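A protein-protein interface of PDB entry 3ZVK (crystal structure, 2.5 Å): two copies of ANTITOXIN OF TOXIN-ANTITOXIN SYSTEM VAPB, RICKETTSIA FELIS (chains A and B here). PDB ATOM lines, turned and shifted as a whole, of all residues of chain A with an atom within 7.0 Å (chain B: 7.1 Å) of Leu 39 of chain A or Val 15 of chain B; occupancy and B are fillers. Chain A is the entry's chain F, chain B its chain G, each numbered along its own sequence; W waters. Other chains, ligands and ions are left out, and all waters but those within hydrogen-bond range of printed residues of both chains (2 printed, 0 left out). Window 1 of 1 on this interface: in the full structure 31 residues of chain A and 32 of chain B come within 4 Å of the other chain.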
ATOM      1  N   PHE A   7      30.358 -12.284  35.557  1.00  0.00           N
ATOM      2  CA  PHE A   7      29.633 -11.888  36.764  1.00  0.00           C
ATOM      3  C   PHE A   7      28.509 -12.885  37.021  1.00  0.00           C
ATOM      4  O   PHE A   7      28.271 -13.762  36.200  1.00  0.00           O
ATOM      5  CB  PHE A   7      29.119 -10.426  36.645  1.00  0.00           C
ATOM      6  CG  PHE A   7      28.039 -10.221  35.613  1.00  0.00           C
ATOM      7  CD1 PHE A   7      28.359 -10.079  34.264  1.00  0.00           C
ATOM      8  CD2 PHE A   7      26.697 -10.202  35.983  1.00  0.00           C
ATOM      9  CE1 PHE A   7      27.358  -9.930  33.305  1.00  0.00           C
ATOM     10  CE2 PHE A   7      25.696 -10.047  35.023  1.00  0.00           C
ATOM     11  CZ  PHE A   7      26.034  -9.910  33.691  1.00  0.00           C
ATOM     12  N   GLN A  13      26.163 -18.000  35.845  1.00  0.00           N
ATOM     13  CA  GLN A  13      27.318 -17.198  35.487  1.00  0.00           C
ATOM     14  C   GLN A  13      26.963 -16.435  34.207  1.00  0.00           C
ATOM     15  O   GLN A  13      26.212 -16.941  33.377  1.00  0.00           O
ATOM     16  CB  GLN A  13      28.497 -18.122  35.210  1.00  0.00           C
ATOM     17  CG  GLN A  13      29.812 -17.493  35.562  1.00  0.00           C
ATOM     18  CD  GLN A  13      30.938 -18.372  35.136  1.00  0.00           C
ATOM     19  OE1 GLN A  13      31.160 -18.604  33.941  1.00  0.00           O
ATOM     20  NE2 GLN A  13      31.678 -18.859  36.108  1.00  0.00           N
ATOM     21  N   ALA A  14      27.486 -15.228  34.036  1.00  0.00           N
ATOM     22  CA  ALA A  14      27.200 -14.449  32.823  1.00  0.00           C
ATOM     23  C   ALA A  14      28.423 -13.688  32.362  1.00  0.00           C
ATOM     24  O   ALA A  14      29.317 -13.427  33.169  1.00  0.00           O
ATOM     25  CB  ALA A  14      26.014 -13.504  33.052  1.00  0.00           C
ATOM     26  N   VAL A  15      28.471 -13.350  31.060  1.00  0.00           N
ATOM     27  CA  VAL A  15      29.561 -12.566  30.441  1.00  0.00           C
ATOM     28  C   VAL A  15      28.979 -11.226  29.971  1.00  0.00           C
ATOM     29  O   VAL A  15      27.990 -11.216  29.254  1.00  0.00           O
ATOM     30  CB  VAL A  15      30.277 -13.341  29.298  1.00  0.00           C
ATOM     31  CG1 VAL A  15      31.383 -12.519  28.662  1.00  0.00           C
ATOM     32  CG2 VAL A  15      30.838 -14.654  29.798  1.00  0.00           C
ATOM     33  N   ARG A  16      29.553 -10.108  30.417  1.00  0.00           N
ATOM     34  CA  ARG A  16      29.072  -8.784  30.024  1.00  0.00           C
ATOM     35  C   ARG A  16      29.711  -8.442  28.687  1.00  0.00           C
ATOM     36  O   ARG A  16      30.933  -8.329  28.614  1.00  0.00           O
ATOM     37  CB  ARG A  16      29.422  -7.744  31.088  1.00  0.00           C
ATOM     38  CG  ARG A  16      28.452  -6.587  31.105  1.00  0.00           C
ATOM     39  CD  ARG A  16      28.848  -5.528  32.121  1.00  0.00           C
ATOM     40  NE  ARG A  16      28.458  -5.921  33.471  1.00  0.00           N
ATOM     41  CZ  ARG A  16      29.301  -6.312  34.420  1.00  0.00           C
ATOM     42  NH1 ARG A  16      30.610  -6.298  34.203  1.00  0.00           N
ATOM     43  NH2 ARG A  16      28.845  -6.702  35.601  1.00  0.00           N
ATOM     44  N   LEU A  17      28.904  -8.349  27.624  1.00  0.00           N
ATOM     45  CA  LEU A  17      29.417  -8.095  26.292  1.00  0.00           C
ATOM     46  C   LEU A  17      29.789  -6.642  26.038  1.00  0.00           C
ATOM     47  O   LEU A  17      28.938  -5.766  26.246  1.00  0.00           O
ATOM     48  CB  LEU A  17      28.400  -8.522  25.207  1.00  0.00           C
ATOM     49  CG  LEU A  17      27.899  -9.967  25.195  1.00  0.00           C
ATOM     50  CD1 LEU A  17      26.799 -10.112  24.169  1.00  0.00           C
ATOM     51  CD2 LEU A  17      29.013 -10.956  24.882  1.00  0.00           C
ATOM     52  N   PHE A  23      24.444  -8.360  20.326  1.00  0.00           N
ATOM     53  CA  PHE A  23      23.622  -9.173  19.434  1.00  0.00           C
ATOM     54  C   PHE A  23      22.282  -8.479  19.242  1.00  0.00           C
ATOM     55  O   PHE A  23      21.834  -7.746  20.131  1.00  0.00           O
ATOM     56  CB  PHE A  23      23.440 -10.574  20.011  1.00  0.00           C
ATOM     57  CG  PHE A  23      24.662 -11.459  19.886  1.00  0.00           C
ATOM     58  CD1 PHE A  23      25.631 -11.488  20.889  1.00  0.00           C
ATOM     59  CD2 PHE A  23      24.828 -12.300  18.781  1.00  0.00           C
ATOM     60  CE1 PHE A  23      26.748 -12.327  20.782  1.00  0.00           C
ATOM     61  CE2 PHE A  23      25.949 -13.140  18.675  1.00  0.00           C
ATOM     62  CZ  PHE A  23      26.898 -13.149  19.675  1.00  0.00           C
ATOM     63  N   VAL A  28      21.184 -17.120  21.523  1.00  0.00           N
ATOM     64  CA  VAL A  28      22.370 -17.491  20.760  1.00  0.00           C
ATOM     65  C   VAL A  28      22.673 -18.957  20.913  1.00  0.00           C
ATOM     66  O   VAL A  28      22.333 -19.568  21.921  1.00  0.00           O
ATOM     67  CB  VAL A  28      23.632 -16.639  21.078  1.00  0.00           C
ATOM     68  CG1 VAL A  28      23.527 -15.227  20.515  1.00  0.00           C
ATOM     69  CG2 VAL A  28      23.985 -16.637  22.567  1.00  0.00           C
ATOM     70  N   SER A  29      23.360 -19.509  19.923  1.00  0.00           N
ATOM     71  CA  SER A  29      23.835 -20.890  19.912  1.00  0.00           C
ATOM     72  C   SER A  29      25.195 -20.903  20.654  1.00  0.00           C
ATOM     73  O   SER A  29      25.991 -19.992  20.458  1.00  0.00           O
ATOM     74  CB  SER A  29      23.993 -21.372  18.469  1.00  0.00           C
ATOM     75  OG  SER A  29      25.283 -21.137  17.911  1.00  0.00           O
ATOM     76  N   VAL A  30      25.447 -21.880  21.521  1.00  0.00           N
ATOM     77  CA  VAL A  30      26.728 -21.996  22.237  1.00  0.00           C
ATOM     78  C   VAL A  30      27.354 -23.320  21.852  1.00  0.00           C
ATOM     79  O   VAL A  30      26.757 -24.368  22.092  1.00  0.00           O
ATOM     80  CB  VAL A  30      26.638 -21.870  23.788  1.00  0.00           C
ATOM     81  CG1 VAL A  30      28.026 -21.812  24.422  1.00  0.00           C
ATOM     82  CG2 VAL A  30      25.801 -20.683  24.211  1.00  0.00           C
ATOM     83  N   ILE A  31      28.554 -23.272  21.265  1.00  0.00           N
ATOM     84  CA  ILE A  31      29.303 -24.444  20.805  1.00  0.00           C
ATOM     85  C   ILE A  31      30.751 -24.412  21.342  1.00  0.00           C
ATOM     86  O   ILE A  31      31.391 -23.369  21.276  1.00  0.00           O
ATOM     87  CB  ILE A  31      29.209 -24.519  19.243  1.00  0.00           C
ATOM     88  CG1 ILE A  31      27.882 -25.178  18.831  1.00  0.00           C
ATOM     89  CG2 ILE A  31      30.379 -25.265  18.589  1.00  0.00           C
ATOM     90  CD1 ILE A  31      27.148 -24.400  17.818  1.00  0.00           C
ATOM     91  N   ILE A  37      34.414 -21.063  23.644  1.00  0.00           N
ATOM     92  CA  ILE A  37      33.097 -21.277  23.048  1.00  0.00           C
ATOM     93  C   ILE A  37      32.814 -20.323  21.900  1.00  0.00           C
ATOM     94  O   ILE A  37      33.283 -19.187  21.910  1.00  0.00           O
ATOM     95  CB  ILE A  37      31.958 -21.169  24.112  1.00  0.00           C
ATOM     96  CG1 ILE A  37      32.029 -19.844  24.911  1.00  0.00           C
ATOM     97  CG2 ILE A  37      31.902 -22.394  25.031  1.00  0.00           C
ATOM     98  CD1 ILE A  37      30.815 -19.505  25.789  1.00  0.00           C
ATOM     99  N   VAL A  38      31.971 -20.755  20.963  1.00  0.00           N
ATOM    100  CA  VAL A  38      31.491 -19.914  19.871  1.00  0.00           C
ATOM    101  C   VAL A  38      30.029 -19.573  20.188  1.00  0.00           C
ATOM    102  O   VAL A  38      29.260 -20.473  20.557  1.00  0.00           O
ATOM    103  CB  VAL A  38      31.613 -20.592  18.474  1.00  0.00           C
ATOM    104  CG1 VAL A  38      31.053 -19.692  17.366  1.00  0.00           C
ATOM    105  CG2 VAL A  38      33.056 -20.953  18.168  1.00  0.00           C
ATOM    106  N   LEU A  39      29.668 -18.281  20.063  1.00  0.00           N
ATOM    107  CA  LEU A  39      28.309 -17.778  20.235  1.00  0.00           C
ATOM    108  C   LEU A  39      27.892 -17.240  18.862  1.00  0.00           C
ATOM    109  O   LEU A  39      28.630 -16.458  18.251  1.00  0.00           O
ATOM    110  CB  LEU A  39      28.186 -16.667  21.319  1.00  0.00           C
ATOM    111  CG  LEU A  39      28.791 -16.839  22.716  1.00  0.00           C
ATOM    112  CD1 LEU A  39      28.496 -15.630  23.534  1.00  0.00           C
ATOM    113  CD2 LEU A  39      28.180 -17.964  23.465  1.00  0.00           C
ATOM    114  N   GLN A  40      26.748 -17.701  18.347  1.00  0.00           N
ATOM    115  CA  GLN A  40      26.237 -17.274  17.038  1.00  0.00           C
ATOM    116  C   GLN A  40      24.758 -16.871  17.128  1.00  0.00           C
ATOM    117  O   GLN A  40      24.014 -17.532  17.852  1.00  0.00           O
ATOM    118  CB  GLN A  40      26.437 -18.365  15.959  1.00  0.00           C
ATOM    119  CG  GLN A  40      27.894 -18.662  15.516  1.00  0.00           C
ATOM    120  CD  GLN A  40      28.711 -17.517  14.922  1.00  0.00           C
ATOM    121  OE1 GLN A  40      29.941 -17.451  15.098  1.00  0.00           O
ATOM    122  NE2 GLN A  40      28.073 -16.617  14.165  1.00  0.00           N
ATOM    123  N   PRO A  41      24.293 -15.814  16.405  1.00  0.00           N
ATOM    124  CA  PRO A  41      22.869 -15.425  16.508  1.00  0.00           C
ATOM    125  C   PRO A  41      21.888 -16.549  16.170  1.00  0.00           C
ATOM    126  O   PRO A  41      21.963 -17.139  15.092  1.00  0.00           O
ATOM    127  CB  PRO A  41      22.737 -14.224  15.559  1.00  0.00           C
ATOM    128  CG  PRO A  41      23.971 -14.231  14.721  1.00  0.00           C
ATOM    129  CD  PRO A  41      25.039 -14.902  15.507  1.00  0.00           C
ATOM    130  N   LYS B   3      21.945 -23.564  23.900  1.00  0.00           N
ATOM    131  CA  LYS B   3      21.478 -22.169  23.785  1.00  0.00           C
ATOM    132  C   LYS B   3      21.739 -21.328  25.034  1.00  0.00           C
ATOM    133  O   LYS B   3      21.705 -21.841  26.151  1.00  0.00           O
ATOM    134  CB  LYS B   3      19.966 -22.127  23.483  1.00  0.00           C
ATOM    135  N   ALA B   4      21.958 -20.030  24.841  1.00  0.00           N
ATOM    136  CA  ALA B   4      22.172 -19.082  25.932  1.00  0.00           C
ATOM    137  C   ALA B   4      21.371 -17.818  25.669  1.00  0.00           C
ATOM    138  O   ALA B   4      21.276 -17.373  24.532  1.00  0.00           O
ATOM    139  CB  ALA B   4      23.642 -18.751  26.076  1.00  0.00           C
ATOM    140  N   LYS B   5      20.763 -17.271  26.718  1.00  0.00           N
ATOM    141  CA  LYS B   5      19.943 -16.068  26.621  1.00  0.00           C
ATOM    142  C   LYS B   5      20.751 -14.793  26.764  1.00  0.00           C
ATOM    143  O   LYS B   5      21.725 -14.734  27.527  1.00  0.00           O
ATOM    144  CB  LYS B   5      18.774 -16.093  27.626  1.00  0.00           C
ATOM    145  CG  LYS B   5      17.712 -17.126  27.268  1.00  0.00           C
ATOM    146  CD  LYS B   5      16.417 -16.968  28.023  1.00  0.00           C
ATOM    147  CE  LYS B   5      15.454 -18.098  27.727  1.00  0.00           C
ATOM    148  NZ  LYS B   5      14.972 -18.117  26.312  1.00  0.00           N
ATOM    149  N   ILE B   6      20.353 -13.775  25.991  1.00  0.00           N
ATOM    150  CA  ILE B   6      20.915 -12.429  26.028  1.00  0.00           C
ATOM    151  C   ILE B   6      19.977 -11.600  26.920  1.00  0.00           C
ATOM    152  O   ILE B   6      18.755 -11.687  26.779  1.00  0.00           O
ATOM    153  CB  ILE B   6      21.109 -11.839  24.603  1.00  0.00           C
ATOM    154  CG1 ILE B   6      22.329 -12.443  23.939  1.00  0.00           C
ATOM    155  CG2 ILE B   6      21.246 -10.331  24.615  1.00  0.00           C
ATOM    156  CD1 ILE B   6      22.088 -12.780  22.575  1.00  0.00           C
ATOM    157  N   PHE B   7      20.548 -10.852  27.872  1.00  0.00           N
ATOM    158  CA  PHE B   7      19.784 -10.017  28.802  1.00  0.00           C
ATOM    159  C   PHE B   7      20.543  -8.717  29.076  1.00  0.00           C
ATOM    160  O   PHE B   7      21.677  -8.574  28.625  1.00  0.00           O
ATOM    161  CB  PHE B   7      19.468 -10.797  30.097  1.00  0.00           C
ATOM    162  CG  PHE B   7      20.664 -11.115  30.962  1.00  0.00           C
ATOM    163  CD1 PHE B   7      21.474 -12.210  30.684  1.00  0.00           C
ATOM    164  CD2 PHE B   7      20.989 -10.309  32.049  1.00  0.00           C
ATOM    165  CE1 PHE B   7      22.601 -12.474  31.455  1.00  0.00           C
ATOM    166  CE2 PHE B   7      22.113 -10.583  32.826  1.00  0.00           C
ATOM    167  CZ  PHE B   7      22.908 -11.665  32.524  1.00  0.00           C
ATOM    168  N   GLN B  13      24.786  -5.224  27.522  1.00  0.00           N
ATOM    169  CA  GLN B  13      24.172  -6.468  27.108  1.00  0.00           C
ATOM    170  C   GLN B  13      24.984  -7.617  27.712  1.00  0.00           C
ATOM    171  O   GLN B  13      26.197  -7.508  27.853  1.00  0.00           O
ATOM    172  CB  GLN B  13      24.220  -6.546  25.592  1.00  0.00           C
ATOM    173  CG  GLN B  13      23.057  -7.288  25.014  1.00  0.00           C
ATOM    174  CD  GLN B  13      23.227  -7.478  23.537  1.00  0.00           C
ATOM    175  OE1 GLN B  13      24.123  -8.185  23.073  1.00  0.00           O
ATOM    176  NE2 GLN B  13      22.372  -6.849  22.766  1.00  0.00           N
ATOM    177  N   ALA B  14      24.337  -8.711  28.073  1.00  0.00           N
ATOM    178  CA  ALA B  14      25.053  -9.856  28.659  1.00  0.00           C
ATOM    179  C   ALA B  14      24.510 -11.169  28.173  1.00  0.00           C
ATOM    180  O   ALA B  14      23.358 -11.218  27.750  1.00  0.00           O
ATOM    181  CB  ALA B  14      25.002  -9.800  30.181  1.00  0.00           C
ATOM    182  N   VAL B  15      25.336 -12.227  28.218  1.00  0.00           N
ATOM    183  CA  VAL B  15      24.975 -13.594  27.826  1.00  0.00           C
ATOM    184  C   VAL B  15      25.006 -14.489  29.076  1.00  0.00           C
ATOM    185  O   VAL B  15      26.001 -14.504  29.801  1.00  0.00           O
ATOM    186  CB  VAL B  15      25.830 -14.150  26.641  1.00  0.00           C
ATOM    187  CG1 VAL B  15      27.336 -14.063  26.903  1.00  0.00           C
ATOM    188  CG2 VAL B  15      25.422 -15.562  26.250  1.00  0.00           C
ATOM    189  N   ARG B  16      23.910 -15.190  29.347  1.00  0.00           N
ATOM    190  CA  ARG B  16      23.848 -16.062  30.514  1.00  0.00           C
ATOM    191  C   ARG B  16      24.379 -17.421  30.100  1.00  0.00           C
ATOM    192  O   ARG B  16      23.782 -18.078  29.250  1.00  0.00           O
ATOM    193  CB  ARG B  16      22.415 -16.172  31.032  1.00  0.00           C
ATOM    194  CG  ARG B  16      22.329 -16.441  32.533  1.00  0.00           C
ATOM    195  CD  ARG B  16      20.903 -16.619  33.025  1.00  0.00           C
ATOM    196  NE  ARG B  16      19.909 -16.029  32.121  1.00  0.00           N
ATOM    197  CZ  ARG B  16      19.254 -14.909  32.344  1.00  0.00           C
ATOM    198  NH1 ARG B  16      19.403 -14.265  33.493  1.00  0.00           N
ATOM    199  NH2 ARG B  16      18.407 -14.441  31.441  1.00  0.00           N
ATOM    200  N   LEU B  17      25.510 -17.832  30.670  1.00  0.00           N
ATOM    201  CA  LEU B  17      26.129 -19.093  30.280  1.00  0.00           C
ATOM    202  C   LEU B  17      25.506 -20.314  30.906  1.00  0.00           C
ATOM    203  O   LEU B  17      25.360 -20.344  32.131  1.00  0.00           O
ATOM    204  CB  LEU B  17      27.643 -19.109  30.605  1.00  0.00           C
ATOM    205  CG  LEU B  17      28.536 -17.992  30.072  1.00  0.00           C
ATOM    206  CD1 LEU B  17      29.889 -18.053  30.720  1.00  0.00           C
ATOM    207  CD2 LEU B  17      28.674 -18.086  28.588  1.00  0.00           C
ATOM    208  N   PRO B  18      25.249 -21.392  30.117  1.00  0.00           N
ATOM    209  CA  PRO B  18      24.808 -22.664  30.728  1.00  0.00           C
ATOM    210  C   PRO B  18      25.926 -23.215  31.636  1.00  0.00           C
ATOM    211  O   PRO B  18      27.099 -22.944  31.375  1.00  0.00           O
ATOM    212  CB  PRO B  18      24.559 -23.574  29.512  1.00  0.00           C
ATOM    213  CG  PRO B  18      24.411 -22.633  28.345  1.00  0.00           C
ATOM    214  CD  PRO B  18      25.384 -21.537  28.654  1.00  0.00           C
ATOM    215  N   LEU B  33      33.933 -13.769  14.935  1.00  0.00           N
ATOM    216  CA  LEU B  33      33.975 -14.903  14.012  1.00  0.00           C
ATOM    217  C   LEU B  33      32.642 -14.892  13.280  1.00  0.00           C
ATOM    218  O   LEU B  33      31.609 -15.248  13.855  1.00  0.00           O
ATOM    219  CB  LEU B  33      34.234 -16.234  14.755  1.00  0.00           C
ATOM    220  CG  LEU B  33      34.458 -17.485  13.918  1.00  0.00           C
ATOM    221  CD1 LEU B  33      35.779 -17.421  13.187  1.00  0.00           C
ATOM    222  CD2 LEU B  33      34.476 -18.708  14.816  1.00  0.00           C
ATOM    223  N   LYS B  35      29.202 -13.678  12.021  1.00  0.00           N
ATOM    224  CA  LYS B  35      28.146 -12.900  12.682  1.00  0.00           C
ATOM    225  C   LYS B  35      28.236 -12.993  14.247  1.00  0.00           C
ATOM    226  O   LYS B  35      27.439 -12.374  14.958  1.00  0.00           O
ATOM    227  CB  LYS B  35      26.761 -13.433  12.226  1.00  0.00           C
ATOM    228  CG  LYS B  35      26.146 -12.700  11.056  1.00  0.00           C
ATOM    229  CD  LYS B  35      24.675 -13.130  10.782  1.00  0.00           C
ATOM    230  CE  LYS B  35      24.446 -14.416   9.993  1.00  0.00           C
ATOM    231  NZ  LYS B  35      25.092 -14.407   8.647  1.00  0.00           N
ATOM    232  N   GLY B  36      29.154 -13.811  14.749  1.00  0.00           N
ATOM    233  CA  GLY B  36      29.274 -14.067  16.171  1.00  0.00           C
ATOM    234  C   GLY B  36      30.617 -13.789  16.794  1.00  0.00           C
ATOM    235  O   GLY B  36      31.396 -12.965  16.306  1.00  0.00           O
ATOM    236  N   ILE B  37      30.873 -14.469  17.910  1.00  0.00           N
ATOM    237  CA  ILE B  37      32.077 -14.263  18.710  1.00  0.00           C
ATOM    238  C   ILE B  37      32.570 -15.545  19.345  1.00  0.00           C
ATOM    239  O   ILE B  37      31.780 -16.443  19.630  1.00  0.00           O
ATOM    240  CB  ILE B  37      31.836 -13.175  19.827  1.00  0.00           C
ATOM    241  CG1 ILE B  37      30.587 -13.505  20.715  1.00  0.00           C
ATOM    242  CG2 ILE B  37      31.780 -11.755  19.255  1.00  0.00           C
ATOM    243  CD1 ILE B  37      30.382 -12.683  21.964  1.00  0.00           C
ATOM    244  N   VAL B  38      33.874 -15.579  19.651  1.00  0.00           N
ATOM    245  CA  VAL B  38      34.504 -16.629  20.434  1.00  0.00           C
ATOM    246  C   VAL B  38      34.824 -16.008  21.816  1.00  0.00           C
ATOM    247  O   VAL B  38      35.346 -14.895  21.866  1.00  0.00           O
ATOM    248  CB  VAL B  38      35.781 -17.229  19.767  1.00  0.00           C
ATOM    249  CG1 VAL B  38      36.407 -18.314  20.646  1.00  0.00           C
ATOM    250  CG2 VAL B  38      35.480 -17.778  18.378  1.00  0.00           C
ATOM    251  N   LEU B  39      34.472 -16.707  22.919  1.00  0.00           N
ATOM    252  CA  LEU B  39      34.832 -16.344  24.301  1.00  0.00           C
ATOM    253  C   LEU B  39      35.778 -17.460  24.756  1.00  0.00           C
ATOM    254  O   LEU B  39      35.461 -18.652  24.611  1.00  0.00           O
ATOM    255  CB  LEU B  39      33.643 -16.265  25.262  1.00  0.00           C
ATOM    256  CG  LEU B  39      32.418 -15.437  24.867  1.00  0.00           C
ATOM    257  CD1 LEU B  39      31.359 -15.552  25.921  1.00  0.00           C
ATOM    258  CD2 LEU B  39      32.755 -13.940  24.697  1.00  0.00           C
HETATM  259  O   HOH W   1      26.066 -20.592  34.704  1.00  0.00           O
HETATM  260  O   HOH W   2      27.128  -3.978  25.785  1.00  0.00           O
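The backbone NH (N) of Ala 14 of chain A lies within hydrogen-bond range of the backbone carbonyl oxygen (O) of Phe 7 of chain A (2.7 Å).
The backbone carbonyl oxygen (O) of Gln 40 of chain A is in hydrogen-bond range of the backbone NH (N) of Ser 29 of chain A (2.9 Å).
The backbone carbonyl oxygen of Ile 31 of chain A is in hydrogen-bond range of the backbone NH of Val 38 of chain A (2.7 Å).
The backbone carbonyl oxygen (O) of Lys 5 of chain B is in hydrogen-bond range of the backbone NH (N) of Arg 16 of chain B, at 2.9 Å.
N of Ala 14 of chain B sits at hydrogen-bond distance from O of Phe 7 of chain B (2.7 Å).
Phe 7 of chain A touches Ala 14 of chain B, and with the chains exchanged Ala 14 of chain A touches Phe 7 of chain B.
Gln 13 of chain A touches Arg 16 of chain B, and with the chains exchanged Arg 16 of chain A touches Gln 13 of chain B.
Ile 37 of chain B touches its own counterpart, Ile 37 of chain A.
Leu 39 of chain A touches Val 15 of chain B, but with the chains exchanged Val 15 of chain A does not touch Leu 39 of chain B (4.01 Å).
Positions printed for both chains: 7, 13, 14, 15, 16, 17, 37, 38 and 39.
Of the 32 pairs that touch across the chains among the printed residues, 18 have their exchanged pair printed and touching as well.
Water W2 bridges the backbone carbonyl oxygen of Leu 17 of chain A (2.6 Å) and the backbone NH of Gln 13 of chain B (3.2 Å).
Water W1 bridges the backbone carbonyl oxygen of Leu 17 of chain B and the backbone NH of Gln 13 of chain A.
Among the printed residues, pairs that only touch across the chains: Ile 37 of chain A with Val 38 of chain B (3.2 Å), Leu 39 of chain A with Gly 36 of chain B (3.2 Å), Ala 14 of chain A with Val 15 of chain B (3.3 Å), Val 15 of chain A with Ala 14 of chain B (3.3 Å), Val 28 of chain A with Lys 3 of chain B (3.3 Å), Val 30 of chain A with Ala 4 of chain B (3.4 Å), Val 38 of chain A with Ile 37 of chain B (3.5 Å), Val 28 of chain A with Ile 6 of chain B (3.5 Å), Pro 41 of chain A with Lys 35 of chain B (3.5 Å), Gln 40 of chain A with Lys 35 of chain B (3.6 Å), Phe 23 of chain A with Ile 6 of chain B (3.6 Å), Val 15 of chain A with Leu 17 of chain B (3.6 Å), Ala 14 of chain A with Phe 7 of chain B (3.6 Å), Leu 17 of chain A with Ile 37 of chain B (3.7 Å), Phe 7 of chain A with Ala 14 of chain B (3.7 Å), Leu 39 of chain A with Leu 39 of chain B (3.7 Å), Arg 16 of chain A with Gln 13 of chain B (3.7 Å), Phe 7 of chain A with Phe 7 of chain B (3.8 Å), Gln 13 of chain A with Arg 16 of chain B (3.8 Å), Ile 37 of chain A with Leu 17 of chain B (3.8 Å), Phe 23 of chain A with Ile 37 of chain B (3.8 Å), Ile 37 of chain A with Ile 37 of chain B (3.9 Å) and Leu 39 of chain A with Val 15 of chain B (3.9 Å).
Hydrophobic or aromatic side chains of chain A that line the printed part of chain B: Phe 7, Ala 14, Val 15, Leu 17, Phe 23, Val 28, Val 30, Ile 37, Leu 39 and Pro 41.
Of the 17 printed residues of chain B, 15 touch a printed residue of chain A.
Printed residues of chain B that touch a printed residue of chain A: Lys 3, Ala 4, Ile 6, Phe 7, Gln 13, Ala 14, Val 15, Arg 16, Leu 17, Leu 33, Lys 35, Gly 36, Ile 37, Val 38 and Leu 39.
Hydrophobic or aromatic side chains of chain B within 4 Å of the printed part of chain A: Ala 4, Ile 6, Phe 7, Ala 14, Val 15, Leu 17, Ile 37, Val 38 and Leu 39.
Among the printed residues, 32 pairs touch across the chains.
Among the printed residues, no Asp or Glu carboxylate lies within 4 Å of a Lys or Arg side-chain nitrogen of the other chain.
Of chain B, only Val 15, Gly 36, Ile 37 and Leu 39 come within 4 Å of Leu 39 of chain A.
Val 15 of chain B touches just these residues of chain A: Ala 14 (3.3 Å), Val 15 (3.0 Å) and Leu 39 (3.9 Å).
Of the printed residues of chain A, Gly 36 of chain B touches Leu 39 (3.2 Å) and Gln 40 (3.1 Å).
Of the printed residues of chain A, Ala 14 of chain B touches Phe 7 (3.7 Å) and Val 15 (3.3 Å).
Printed residues of chain B within 4 Å of Val 28 of chain A: Lys 3 (3.3 Å), Ala 4 (3.0 Å) and Ile 6 (3.5 Å).
Of the printed residues of chain B, Val 15 of chain A touches Ala 14 (3.3 Å), Val 15 (3.0 Å) and Leu 17 (3.6 Å).
The nearest residue of chain B that does not touch Leu 39 of chain A is Val 38 of chain B (5.0 Å).
The nearest printed residue of chain A that does not touch Val 15 of chain B is Leu 17 of chain A (4.1 Å).
O of Gln 13 of chain A is in hydrogen-bond range of N of Leu 17 of chain B (2.9 Å).
N of Val 15 of chain A lies within hydrogen-bond range of O of Val 15 of chain B (3.0 Å).
The backbone NH (N) of Leu 17 of chain A lies within hydrogen-bond range of the backbone carbonyl oxygen (O) of Gln 13 of chain B.
OE1 of Gln 13 of chain B lies within hydrogen-bond range of N of Phe 23 of chain A, 2.8 Å away.
The backbone carbonyl oxygen (O) of Val 28 of chain A is in hydrogen-bond range of the backbone NH (N) of Ala 4 of chain B, at 3.0 Å.
The backbone carbonyl oxygen of Leu 39 of chain B lies within hydrogen-bond range of the backbone NH of Ile 37 of chain A (2.8 Å).
N of Leu 39 of chain A sits at hydrogen-bond distance from O of Ile 37 of chain B (2.8 Å).
The backbone carbonyl oxygen (O) of Leu 33 of chain B lies close to the side-chain amide oxygen (OE1) of Gln 40 of chain A.
The side-chain amide nitrogen (NE2) of Gln 40 of chain A lies close to the backbone NH (N) of Gly 36 of chain B (3.1 Å).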
